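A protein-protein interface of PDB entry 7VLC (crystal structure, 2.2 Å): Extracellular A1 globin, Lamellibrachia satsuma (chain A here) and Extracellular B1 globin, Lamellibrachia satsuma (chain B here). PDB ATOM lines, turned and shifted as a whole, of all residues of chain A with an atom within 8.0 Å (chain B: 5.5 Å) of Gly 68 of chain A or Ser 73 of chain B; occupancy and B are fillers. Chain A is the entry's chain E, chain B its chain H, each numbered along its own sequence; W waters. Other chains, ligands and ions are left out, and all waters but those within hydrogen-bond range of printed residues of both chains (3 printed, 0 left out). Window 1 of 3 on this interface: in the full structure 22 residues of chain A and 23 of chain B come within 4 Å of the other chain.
The backbone NH (N) of Arg 65 of chain A lies close to the side-chain sulfur (SD) of Met 77 of chain B, 3.8 Å away.
The side-chain hydroxyl (OG) of Ser 73 of chain B sits at hydrogen-bond distance from the backbone carbonyl oxygen (O) of Gly 68 of chain A, 3.4 Å away.
The side-chain carboxylate of Asp 76 of chain B lies within salt-bridge range of the guanidinium group of Arg 24 of chain A (3.1 Å).
SD of Met 77 of chain B lies close to O of Ala 64 of chain A, at 3.5 Å.
The guanidinium group of Arg 70 of chain B lies within salt-bridge range of the side-chain carboxylate of Asp 86 of chain A (2.7 Å).
The backbone carbonyl oxygen (O) of Arg 72 of chain A sits at hydrogen-bond distance from the side-chain hydroxyl (OG) of Ser 75 of chain A (2.8 Å).
OD2 of Asp 86 of chain A lies within salt-bridge range of NE of Arg 72 of chain A.
Among the printed residues, merely in contact across the chains: Arg 72 of chain A with Val 69 of chain B (3.7 Å) and Arg 72 of chain A with Arg 70 of chain B (3.4 Å).
Tyr 18 of chain A touches none of the printed residues of chain B.
Printed residues of chain B within 4 Å of Arg 65 of chain A: Met 77.
Of chain B, only Ser 73 comes within 4 Å of Gly 68 of chain A.
Printed residues of chain A within 4 Å of Val 69 of chain B: Arg 72.
Of chain A, only Gly 68 comes within 4 Å of Ser 73 of chain B.
No residue of chain A comes within 4 Å of Gly 74 of chain B.
Of the printed residues of chain A, Asp 76 of chain B touches Arg 24 (3.1 Å).
Printed residues of chain A within 4 Å of Met 77 of chain B: Ala 64 (3.5 Å) and Arg 65 (3.7 Å).
The nearest residue of chain B that does not touch Gly 68 of chain A is Met 77 of chain B (5.3 Å).
The nearest residue of chain A that does not touch Ser 73 of chain B is Arg 72 of chain A (4.3 Å).
The nearest printed residue of chain B that does not touch Arg 65 of chain A is Ser 73 of chain B (6.2 Å).
Of the 12 printed residues of chain B, 5 touch a printed residue of chain A.
Printed residues of chain B that touch a printed residue of chain A: Val 69, Arg 70, Ser 73, Asp 76 and Met 77.
Hydrophobic or aromatic side chains of chain B that line the printed part of chain A: Val 69 and Met 77.
Among the printed residues, Asp or Glu carboxylates within 4 Å of a Lys or Arg side-chain nitrogen of the other chain: Arg 24 of chain A with Asp 76 of chain B and Asp 86 of chain A with Arg 70 of chain B.
Water W1 bridges NH1 of Arg 24 of chain A and OD1 of Asp 76 of chain B.
Water W3 lies within hydrogen-bond range of OG of Ser 73 of chain B (2.6 Å) and NH1 of Arg 72 of chain A (3.1 Å).
Water W2 lies within hydrogen-bond range of OH of Tyr 20 of chain B (2.6 Å), OG of Ser 73 of chain B (2.8 Å) and OD2 of Asp 71 of chain A (2.9 Å).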
ATOM      1  N   TRP A  14      22.308  17.401  -0.245  1.00  0.00           N
ATOM      2  CA  TRP A  14      22.202  15.950  -0.377  1.00  0.00           C
ATOM      3  C   TRP A  14      21.982  15.549  -1.831  1.00  0.00           C
ATOM      4  O   TRP A  14      22.700  14.697  -2.365  1.00  0.00           O
ATOM      5  CB  TRP A  14      21.069  15.419   0.501  1.00  0.00           C
ATOM      6  CG  TRP A  14      20.678  14.004   0.174  1.00  0.00           C
ATOM      7  CD1 TRP A  14      19.600  13.599  -0.563  1.00  0.00           C
ATOM      8  CD2 TRP A  14      21.370  12.813   0.562  1.00  0.00           C
ATOM      9  NE1 TRP A  14      19.578  12.225  -0.652  1.00  0.00           N
ATOM     10  CE2 TRP A  14      20.654  11.720   0.032  1.00  0.00           C
ATOM     11  CE3 TRP A  14      22.524  12.564   1.311  1.00  0.00           C
ATOM     12  CZ2 TRP A  14      21.056  10.397   0.227  1.00  0.00           C
ATOM     13  CZ3 TRP A  14      22.922  11.255   1.503  1.00  0.00           C
ATOM     14  CH2 TRP A  14      22.190  10.186   0.964  1.00  0.00           C
ATOM     15  N   TYR A  18      24.486  13.161  -3.725  1.00  0.00           N
ATOM     16  CA  TYR A  18      23.979  11.800  -3.881  1.00  0.00           C
ATOM     17  C   TYR A  18      24.149  11.309  -5.315  1.00  0.00           C
ATOM     18  O   TYR A  18      24.700  10.227  -5.550  1.00  0.00           O
ATOM     19  CB  TYR A  18      22.513  11.752  -3.451  1.00  0.00           C
ATOM     20  CG  TYR A  18      21.896  10.376  -3.418  1.00  0.00           C
ATOM     21  CD1 TYR A  18      22.548   9.313  -2.817  1.00  0.00           C
ATOM     22  CD2 TYR A  18      20.641  10.150  -3.965  1.00  0.00           C
ATOM     23  CE1 TYR A  18      21.978   8.058  -2.777  1.00  0.00           C
ATOM     24  CE2 TYR A  18      20.061   8.902  -3.926  1.00  0.00           C
ATOM     25  CZ  TYR A  18      20.732   7.861  -3.332  1.00  0.00           C
ATOM     26  OH  TYR A  18      20.147   6.616  -3.299  1.00  0.00           O
ATOM     27  N   ARG A  24      25.479   6.620  -6.788  1.00  0.00           N
ATOM     28  CA  ARG A  24      24.897   6.340  -5.480  1.00  0.00           C
ATOM     29  C   ARG A  24      25.592   5.166  -4.807  1.00  0.00           C
ATOM     30  O   ARG A  24      25.852   5.204  -3.597  1.00  0.00           O
ATOM     31  CB  ARG A  24      23.400   6.064  -5.617  1.00  0.00           C
ATOM     32  CG  ARG A  24      22.654   7.123  -6.399  1.00  0.00           C
ATOM     33  CD  ARG A  24      21.211   6.728  -6.607  1.00  0.00           C
ATOM     34  NE  ARG A  24      20.497   7.693  -7.435  1.00  0.00           N
ATOM     35  CZ  ARG A  24      19.226   7.561  -7.793  1.00  0.00           C
ATOM     36  NH1 ARG A  24      18.533   6.503  -7.394  1.00  0.00           N
ATOM     37  NH2 ARG A  24      18.650   8.485  -8.546  1.00  0.00           N
ATOM     38  N   ALA A  61      23.562  -4.599  -0.896  1.00  0.00           N
ATOM     39  CA  ALA A  61      22.122  -4.410  -0.768  1.00  0.00           C
ATOM     40  C   ALA A  61      21.783  -3.635   0.499  1.00  0.00           C
ATOM     41  O   ALA A  61      20.855  -2.816   0.504  1.00  0.00           O
ATOM     42  CB  ALA A  61      21.416  -5.767  -0.784  1.00  0.00           C
ATOM     43  N   HIS A  62      22.523  -3.879   1.583  1.00  0.00           N
ATOM     44  CA  HIS A  62      22.311  -3.120   2.809  1.00  0.00           C
ATOM     45  C   HIS A  62      22.689  -1.658   2.609  1.00  0.00           C
ATOM     46  O   HIS A  62      21.961  -0.756   3.043  1.00  0.00           O
ATOM     47  CB  HIS A  62      23.120  -3.731   3.953  1.00  0.00           C
ATOM     48  CG  HIS A  62      23.092  -2.918   5.210  1.00  0.00           C
ATOM     49  ND1 HIS A  62      21.986  -2.855   6.031  1.00  0.00           N
ATOM     50  CD2 HIS A  62      24.028  -2.121   5.778  1.00  0.00           C
ATOM     51  CE1 HIS A  62      22.244  -2.059   7.053  1.00  0.00           C
ATOM     52  NE2 HIS A  62      23.476  -1.600   6.923  1.00  0.00           N
ATOM     53  N   ILE A  63      23.824  -1.413   1.948  1.00  0.00           N
ATOM     54  CA  ILE A  63      24.231  -0.053   1.612  1.00  0.00           C
ATOM     55  C   ILE A  63      23.119   0.657   0.852  1.00  0.00           C
ATOM     56  O   ILE A  63      22.766   1.800   1.160  1.00  0.00           O
ATOM     57  CB  ILE A  63      25.539  -0.071   0.802  1.00  0.00           C
ATOM     58  CG1 ILE A  63      26.705  -0.544   1.672  1.00  0.00           C
ATOM     59  CG2 ILE A  63      25.820   1.300   0.222  1.00  0.00           C
ATOM     60  CD1 ILE A  63      28.030  -0.585   0.938  1.00  0.00           C
ATOM     61  N   ALA A  64      22.538  -0.020  -0.143  1.00  0.00           N
ATOM     62  CA  ALA A  64      21.472   0.599  -0.924  1.00  0.00           C
ATOM     63  C   ALA A  64      20.259   0.916  -0.058  1.00  0.00           C
ATOM     64  O   ALA A  64      19.629   1.967  -0.227  1.00  0.00           O
ATOM     65  CB  ALA A  64      21.080  -0.306  -2.093  1.00  0.00           C
ATOM     66  N   ARG A  65      19.923   0.025   0.882  1.00  0.00           N
ATOM     67  CA  ARG A  65      18.777   0.265   1.758  1.00  0.00           C
ATOM     68  C   ARG A  65      19.015   1.458   2.679  1.00  0.00           C
ATOM     69  O   ARG A  65      18.094   2.247   2.928  1.00  0.00           O
ATOM     70  CB  ARG A  65      18.459  -0.990   2.580  1.00  0.00           C
ATOM     71  CG  ARG A  65      17.743  -2.081   1.794  1.00  0.00           C
ATOM     72  CD  ARG A  65      17.212  -3.197   2.692  1.00  0.00           C
ATOM     73  NE  ARG A  65      18.281  -3.988   3.299  1.00  0.00           N
ATOM     74  CZ  ARG A  65      18.841  -5.052   2.729  1.00  0.00           C
ATOM     75  NH1 ARG A  65      18.442  -5.457   1.531  1.00  0.00           N
ATOM     76  NH2 ARG A  65      19.810  -5.708   3.354  1.00  0.00           N
ATOM     77  N   VAL A  66      20.242   1.617   3.180  1.00  0.00           N
ATOM     78  CA  VAL A  66      20.531   2.692   4.127  1.00  0.00           C
ATOM     79  C   VAL A  66      20.504   4.051   3.433  1.00  0.00           C
ATOM     80  O   VAL A  66      19.854   4.993   3.903  1.00  0.00           O
ATOM     81  CB  VAL A  66      21.879   2.447   4.826  1.00  0.00           C
ATOM     82  CG1 VAL A  66      22.259   3.658   5.665  1.00  0.00           C
ATOM     83  CG2 VAL A  66      21.806   1.184   5.685  1.00  0.00           C
ATOM     84  N   ILE A  67      21.225   4.187   2.315  1.00  0.00           N
ATOM     85  CA  ILE A  67      21.219   5.465   1.611  1.00  0.00           C
ATOM     86  C   ILE A  67      19.867   5.717   0.957  1.00  0.00           C
ATOM     87  O   ILE A  67      19.514   6.872   0.695  1.00  0.00           O
ATOM     88  CB  ILE A  67      22.368   5.539   0.585  1.00  0.00           C
ATOM     89  CG1 ILE A  67      22.097   4.626  -0.608  1.00  0.00           C
ATOM     90  CG2 ILE A  67      23.698   5.172   1.235  1.00  0.00           C
ATOM     91  CD1 ILE A  67      23.215   4.615  -1.622  1.00  0.00           C
ATOM     92  N   GLY A  68      19.089   4.665   0.702  1.00  0.00           N
ATOM     93  CA  GLY A  68      17.706   4.871   0.315  1.00  0.00           C
ATOM     94  C   GLY A  68      16.855   5.398   1.454  1.00  0.00           C
ATOM     95  O   GLY A  68      15.944   6.201   1.229  1.00  0.00           O
ATOM     96  N   GLY A  69      17.135   4.961   2.682  1.00  0.00           N
ATOM     97  CA  GLY A  69      16.445   5.524   3.833  1.00  0.00           C
ATOM     98  C   GLY A  69      16.846   6.964   4.103  1.00  0.00           C
ATOM     99  O   GLY A  69      16.000   7.804   4.416  1.00  0.00           O
ATOM    100  N   LEU A  70      18.141   7.268   3.994  1.00  0.00           N
ATOM    101  CA  LEU A  70      18.579   8.656   4.110  1.00  0.00           C
ATOM    102  C   LEU A  70      17.904   9.537   3.063  1.00  0.00           C
ATOM    103  O   LEU A  70      17.414  10.625   3.383  1.00  0.00           O
ATOM    104  CB  LEU A  70      20.101   8.742   3.982  1.00  0.00           C
ATOM    105  CG  LEU A  70      20.944   8.279   5.169  1.00  0.00           C
ATOM    106  CD1 LEU A  70      22.414   8.217   4.779  1.00  0.00           C
ATOM    107  CD2 LEU A  70      20.745   9.196   6.369  1.00  0.00           C
ATOM    108  N   ASP A  71      17.855   9.075   1.809  1.00  0.00           N
ATOM    109  CA  ASP A  71      17.271   9.879   0.738  1.00  0.00           C
ATOM    110  C   ASP A  71      15.788  10.140   0.970  1.00  0.00           C
ATOM    111  O   ASP A  71      15.301  11.250   0.722  1.00  0.00           O
ATOM    112  CB  ASP A  71      17.477   9.191  -0.612  1.00  0.00           C
ATOM    113  CG  ASP A  71      16.896   9.991  -1.765  1.00  0.00           C
ATOM    114  OD1 ASP A  71      17.486  11.029  -2.120  1.00  0.00           O
ATOM    115  OD2 ASP A  71      15.848   9.584  -2.317  1.00  0.00           O
ATOM    116  N   ARG A  72      15.045   9.128   1.423  1.00  0.00           N
ATOM    117  CA  ARG A  72      13.611   9.318   1.606  1.00  0.00           C
ATOM    118  C   ARG A  72      13.303  10.132   2.858  1.00  0.00           C
ATOM    119  O   ARG A  72      12.338  10.904   2.862  1.00  0.00           O
ATOM    120  CB  ARG A  72      12.890   7.964   1.645  1.00  0.00           C
ATOM    121  CG  ARG A  72      13.129   7.132   2.900  1.00  0.00           C
ATOM    122  CD  ARG A  72      12.332   5.832   2.858  1.00  0.00           C
ATOM    123  NE  ARG A  72      12.004   5.346   4.198  1.00  0.00           N
ATOM    124  CZ  ARG A  72      12.437   4.199   4.714  1.00  0.00           C
ATOM    125  NH1 ARG A  72      13.214   3.394   4.002  1.00  0.00           N
ATOM    126  NH2 ARG A  72      12.076   3.852   5.940  1.00  0.00           N
ATOM    127  N   VAL A  73      14.115   9.996   3.907  1.00  0.00           N
ATOM    128  CA  VAL A  73      13.942  10.821   5.100  1.00  0.00           C
ATOM    129  C   VAL A  73      14.239  12.284   4.782  1.00  0.00           C
ATOM    130  O   VAL A  73      13.483  13.185   5.159  1.00  0.00           O
ATOM    131  CB  VAL A  73      14.827  10.301   6.246  1.00  0.00           C
ATOM    132  CG1 VAL A  73      14.926  11.338   7.347  1.00  0.00           C
ATOM    133  CG2 VAL A  73      14.273   8.990   6.800  1.00  0.00           C
ATOM    134  N   ILE A  74      15.343  12.537   4.074  1.00  0.00           N
ATOM    135  CA  ILE A  74      15.722  13.907   3.735  1.00  0.00           C
ATOM    136  C   ILE A  74      14.672  14.542   2.833  1.00  0.00           C
ATOM    137  O   ILE A  74      14.356  15.730   2.966  1.00  0.00           O
ATOM    138  CB  ILE A  74      17.125  13.922   3.095  1.00  0.00           C
ATOM    139  CG1 ILE A  74      18.184  13.572   4.143  1.00  0.00           C
ATOM    140  CG2 ILE A  74      17.425  15.268   2.451  1.00  0.00           C
ATOM    141  CD1 ILE A  74      19.582  13.497   3.594  1.00  0.00           C
ATOM    142  N   SER A  75      14.089  13.755   1.924  1.00  0.00           N
ATOM    143  CA  SER A  75      13.073  14.305   1.034  1.00  0.00           C
ATOM    144  C   SER A  75      11.829  14.741   1.798  1.00  0.00           C
ATOM    145  O   SER A  75      11.158  15.695   1.389  1.00  0.00           O
ATOM    146  CB  SER A  75      12.699  13.290  -0.046  1.00  0.00           C
ATOM    147  OG  SER A  75      11.807  12.310   0.458  1.00  0.00           O
ATOM    148  N   MET A  76      11.509  14.070   2.903  1.00  0.00           N
ATOM    149  CA  MET A  76      10.343  14.399   3.713  1.00  0.00           C
ATOM    150  C   MET A  76      10.650  15.395   4.826  1.00  0.00           C
ATOM    151  O   MET A  76       9.826  15.566   5.728  1.00  0.00           O
ATOM    152  CB  MET A  76       9.744  13.127   4.320  1.00  0.00           C
ATOM    153  CG  MET A  76       9.073  12.202   3.320  1.00  0.00           C
ATOM    154  SD  MET A  76       8.436  10.708   4.103  1.00  0.00           S
ATOM    155  CE  MET A  76       9.955  10.013   4.749  1.00  0.00           C
ATOM    156  N   ASP A  86       7.897   8.073   9.273  1.00  0.00           N
ATOM    157  CA  ASP A  86       8.974   7.227   8.765  1.00  0.00           C
ATOM    158  C   ASP A  86      10.080   7.038   9.797  1.00  0.00           C
ATOM    159  O   ASP A  86      10.650   5.946   9.903  1.00  0.00           O
ATOM    160  CB  ASP A  86       9.549   7.818   7.476  1.00  0.00           C
ATOM    161  CG  ASP A  86      10.163   6.762   6.571  1.00  0.00           C
ATOM    162  OD1 ASP A  86       9.811   5.573   6.712  1.00  0.00           O
ATOM    163  OD2 ASP A  86      11.002   7.116   5.719  1.00  0.00           O
ATOM    164  N   LEU A  90      11.397   3.592  11.107  1.00  0.00           N
ATOM    165  CA  LEU A  90      12.804   3.211  11.207  1.00  0.00           C
ATOM    166  C   LEU A  90      13.185   2.879  12.644  1.00  0.00           C
ATOM    167  O   LEU A  90      14.001   1.980  12.884  1.00  0.00           O
ATOM    168  CB  LEU A  90      13.689   4.335  10.668  1.00  0.00           C
ATOM    169  CG  LEU A  90      13.598   4.617   9.168  1.00  0.00           C
ATOM    170  CD1 LEU A  90      14.263   5.944   8.820  1.00  0.00           C
ATOM    171  CD2 LEU A  90      14.234   3.478   8.394  1.00  0.00           C
ATOM    172  N   TYR B  20      11.994  10.452 -10.918  1.00  0.00           N
ATOM    173  CA  TYR B  20      12.336  10.128  -9.538  1.00  0.00           C
ATOM    174  C   TYR B  20      13.843  10.210  -9.381  1.00  0.00           C
ATOM    175  O   TYR B  20      14.579   9.517 -10.092  1.00  0.00           O
ATOM    176  CB  TYR B  20      11.835   8.730  -9.158  1.00  0.00           C
ATOM    177  CG  TYR B  20      12.006   8.392  -7.689  1.00  0.00           C
ATOM    178  CD1 TYR B  20      13.257   8.071  -7.168  1.00  0.00           C
ATOM    179  CD2 TYR B  20      10.916   8.383  -6.828  1.00  0.00           C
ATOM    180  CE1 TYR B  20      13.419   7.769  -5.832  1.00  0.00           C
ATOM    181  CE2 TYR B  20      11.069   8.071  -5.486  1.00  0.00           C
ATOM    182  CZ  TYR B  20      12.323   7.765  -4.996  1.00  0.00           C
ATOM    183  OH  TYR B  20      12.491   7.454  -3.668  1.00  0.00           O
ATOM    184  N   THR B  68       3.973   5.058   0.906  1.00  0.00           N
ATOM    185  CA  THR B  68       4.220   5.109  -0.531  1.00  0.00           C
ATOM    186  C   THR B  68       5.621   5.621  -0.835  1.00  0.00           C
ATOM    187  O   THR B  68       6.229   5.209  -1.830  1.00  0.00           O
ATOM    188  CB  THR B  68       3.175   5.981  -1.225  1.00  0.00           C
ATOM    189  OG1 THR B  68       3.332   7.337  -0.810  1.00  0.00           O
ATOM    190  CG2 THR B  68       1.769   5.504  -0.878  1.00  0.00           C
ATOM    191  N   VAL B  69       6.151   6.514   0.007  1.00  0.00           N
ATOM    192  CA  VAL B  69       7.537   6.943  -0.142  1.00  0.00           C
ATOM    193  C   VAL B  69       8.484   5.774   0.115  1.00  0.00           C
ATOM    194  O   VAL B  69       9.504   5.622  -0.570  1.00  0.00           O
ATOM    195  CB  VAL B  69       7.827   8.138   0.787  1.00  0.00           C
ATOM    196  CG1 VAL B  69       9.315   8.413   0.866  1.00  0.00           C
ATOM    197  CG2 VAL B  69       7.101   9.375   0.290  1.00  0.00           C
ATOM    198  N   ARG B  70       8.151   4.916   1.084  1.00  0.00           N
ATOM    199  CA  ARG B  70       8.939   3.706   1.298  1.00  0.00           C
ATOM    200  C   ARG B  70       8.859   2.776   0.093  1.00  0.00           C
ATOM    201  O   ARG B  70       9.866   2.181  -0.310  1.00  0.00           O
ATOM    202  CB  ARG B  70       8.461   2.979   2.555  1.00  0.00           C
ATOM    203  CG  ARG B  70       9.245   3.308   3.806  1.00  0.00           C
ATOM    204  CD  ARG B  70       8.700   2.573   5.029  1.00  0.00           C
ATOM    205  NE  ARG B  70       8.223   3.527   6.026  1.00  0.00           N
ATOM    206  CZ  ARG B  70       6.948   3.700   6.355  1.00  0.00           C
ATOM    207  NH1 ARG B  70       6.003   2.960   5.790  1.00  0.00           N
ATOM    208  NH2 ARG B  70       6.621   4.608   7.263  1.00  0.00           N
ATOM    209  N   VAL B  71       7.668   2.637  -0.495  1.00  0.00           N
ATOM    210  CA  VAL B  71       7.499   1.738  -1.633  1.00  0.00           C
ATOM    211  C   VAL B  71       8.251   2.268  -2.848  1.00  0.00           C
ATOM    212  O   VAL B  71       8.979   1.527  -3.519  1.00  0.00           O
ATOM    213  CB  VAL B  71       6.004   1.537  -1.937  1.00  0.00           C
ATOM    214  CG1 VAL B  71       5.816   0.636  -3.157  1.00  0.00           C
ATOM    215  CG2 VAL B  71       5.291   0.958  -0.728  1.00  0.00           C
ATOM    216  N   LEU B  72       8.091   3.559  -3.148  1.00  0.00           N
ATOM    217  CA  LEU B  72       8.772   4.140  -4.301  1.00  0.00           C
ATOM    218  C   LEU B  72      10.286   4.084  -4.141  1.00  0.00           C
ATOM    219  O   LEU B  72      11.011   3.887  -5.122  1.00  0.00           O
ATOM    220  CB  LEU B  72       8.309   5.579  -4.516  1.00  0.00           C
ATOM    221  CG  LEU B  72       6.863   5.751  -4.980  1.00  0.00           C
ATOM    222  CD1 LEU B  72       6.568   7.219  -5.138  1.00  0.00           C
ATOM    223  CD2 LEU B  72       6.588   5.002  -6.284  1.00  0.00           C
ATOM    224  N   SER B  73      10.784   4.266  -2.916  1.00  0.00           N
ATOM    225  CA  SER B  73      12.220   4.145  -2.686  1.00  0.00           C
ATOM    226  C   SER B  73      12.693   2.716  -2.926  1.00  0.00           C
ATOM    227  O   SER B  73      13.800   2.500  -3.431  1.00  0.00           O
ATOM    228  CB  SER B  73      12.574   4.598  -1.268  1.00  0.00           C
ATOM    229  OG  SER B  73      13.978   4.568  -1.062  1.00  0.00           O
ATOM    230  N   GLY B  74      11.866   1.729  -2.577  1.00  0.00           N
ATOM    231  CA  GLY B  74      12.213   0.352  -2.884  1.00  0.00           C
ATOM    232  C   GLY B  74      12.200   0.070  -4.375  1.00  0.00           C
ATOM    233  O   GLY B  74      13.060  -0.651  -4.886  1.00  0.00           O
ATOM    234  N   LEU B  75      11.225   0.632  -5.091  1.00  0.00           N
ATOM    235  CA  LEU B  75      11.191   0.479  -6.541  1.00  0.00           C
ATOM    236  C   LEU B  75      12.387   1.162  -7.191  1.00  0.00           C
ATOM    237  O   LEU B  75      13.013   0.603  -8.101  1.00  0.00           O
ATOM    238  CB  LEU B  75       9.884   1.043  -7.097  1.00  0.00           C
ATOM    239  CG  LEU B  75       9.686   0.922  -8.607  1.00  0.00           C
ATOM    240  CD1 LEU B  75       9.740  -0.535  -9.050  1.00  0.00           C
ATOM    241  CD2 LEU B  75       8.369   1.542  -9.012  1.00  0.00           C
ATOM    242  N   ASP B  76      12.716   2.374  -6.733  1.00  0.00           N
ATOM    243  CA  ASP B  76      13.885   3.080  -7.245  1.00  0.00           C
ATOM    244  C   ASP B  76      15.163   2.305  -6.964  1.00  0.00           C
ATOM    245  O   ASP B  76      16.094   2.304  -7.777  1.00  0.00           O
ATOM    246  CB  ASP B  76      13.959   4.477  -6.628  1.00  0.00           C
ATOM    247  CG  ASP B  76      15.331   5.107  -6.772  1.00  0.00           C
ATOM    248  OD1 ASP B  76      16.209   4.844  -5.919  1.00  0.00           O
ATOM    249  OD2 ASP B  76      15.532   5.850  -7.752  1.00  0.00           O
ATOM    250  N   MET B  77      15.218   1.640  -5.812  1.00  0.00           N
ATOM    251  CA  MET B  77      16.375   0.829  -5.463  1.00  0.00           C
ATOM    252  C   MET B  77      16.534  -0.345  -6.424  1.00  0.00           C
ATOM    253  O   MET B  77      17.638  -0.629  -6.902  1.00  0.00           O
ATOM    254  CB  MET B  77      16.216   0.339  -4.030  1.00  0.00           C
ATOM    255  CG  MET B  77      17.485   0.112  -3.281  1.00  0.00           C
ATOM    256  SD  MET B  77      17.060  -0.098  -1.545  1.00  0.00           S
ATOM    257  CE  MET B  77      15.792  -1.364  -1.639  1.00  0.00           C
ATOM    258  N   GLY B  78      15.433  -1.041  -6.721  1.00  0.00           N
ATOM    259  CA  GLY B  78      15.502  -2.168  -7.638  1.00  0.00           C
ATOM    260  C   GLY B  78      15.824  -1.761  -9.062  1.00  0.00           C
ATOM    261  O   GLY B  78      16.543  -2.474  -9.770  1.00  0.00           O
HETATM  262  O   HOH W   1      18.981   4.239  -6.415  1.00  0.00           O
HETATM  263  O   HOH W   2      14.746   6.913  -2.403  1.00  0.00           O
HETATM  264  O   HOH W   3      14.248   3.108   1.111  1.00  0.00           O
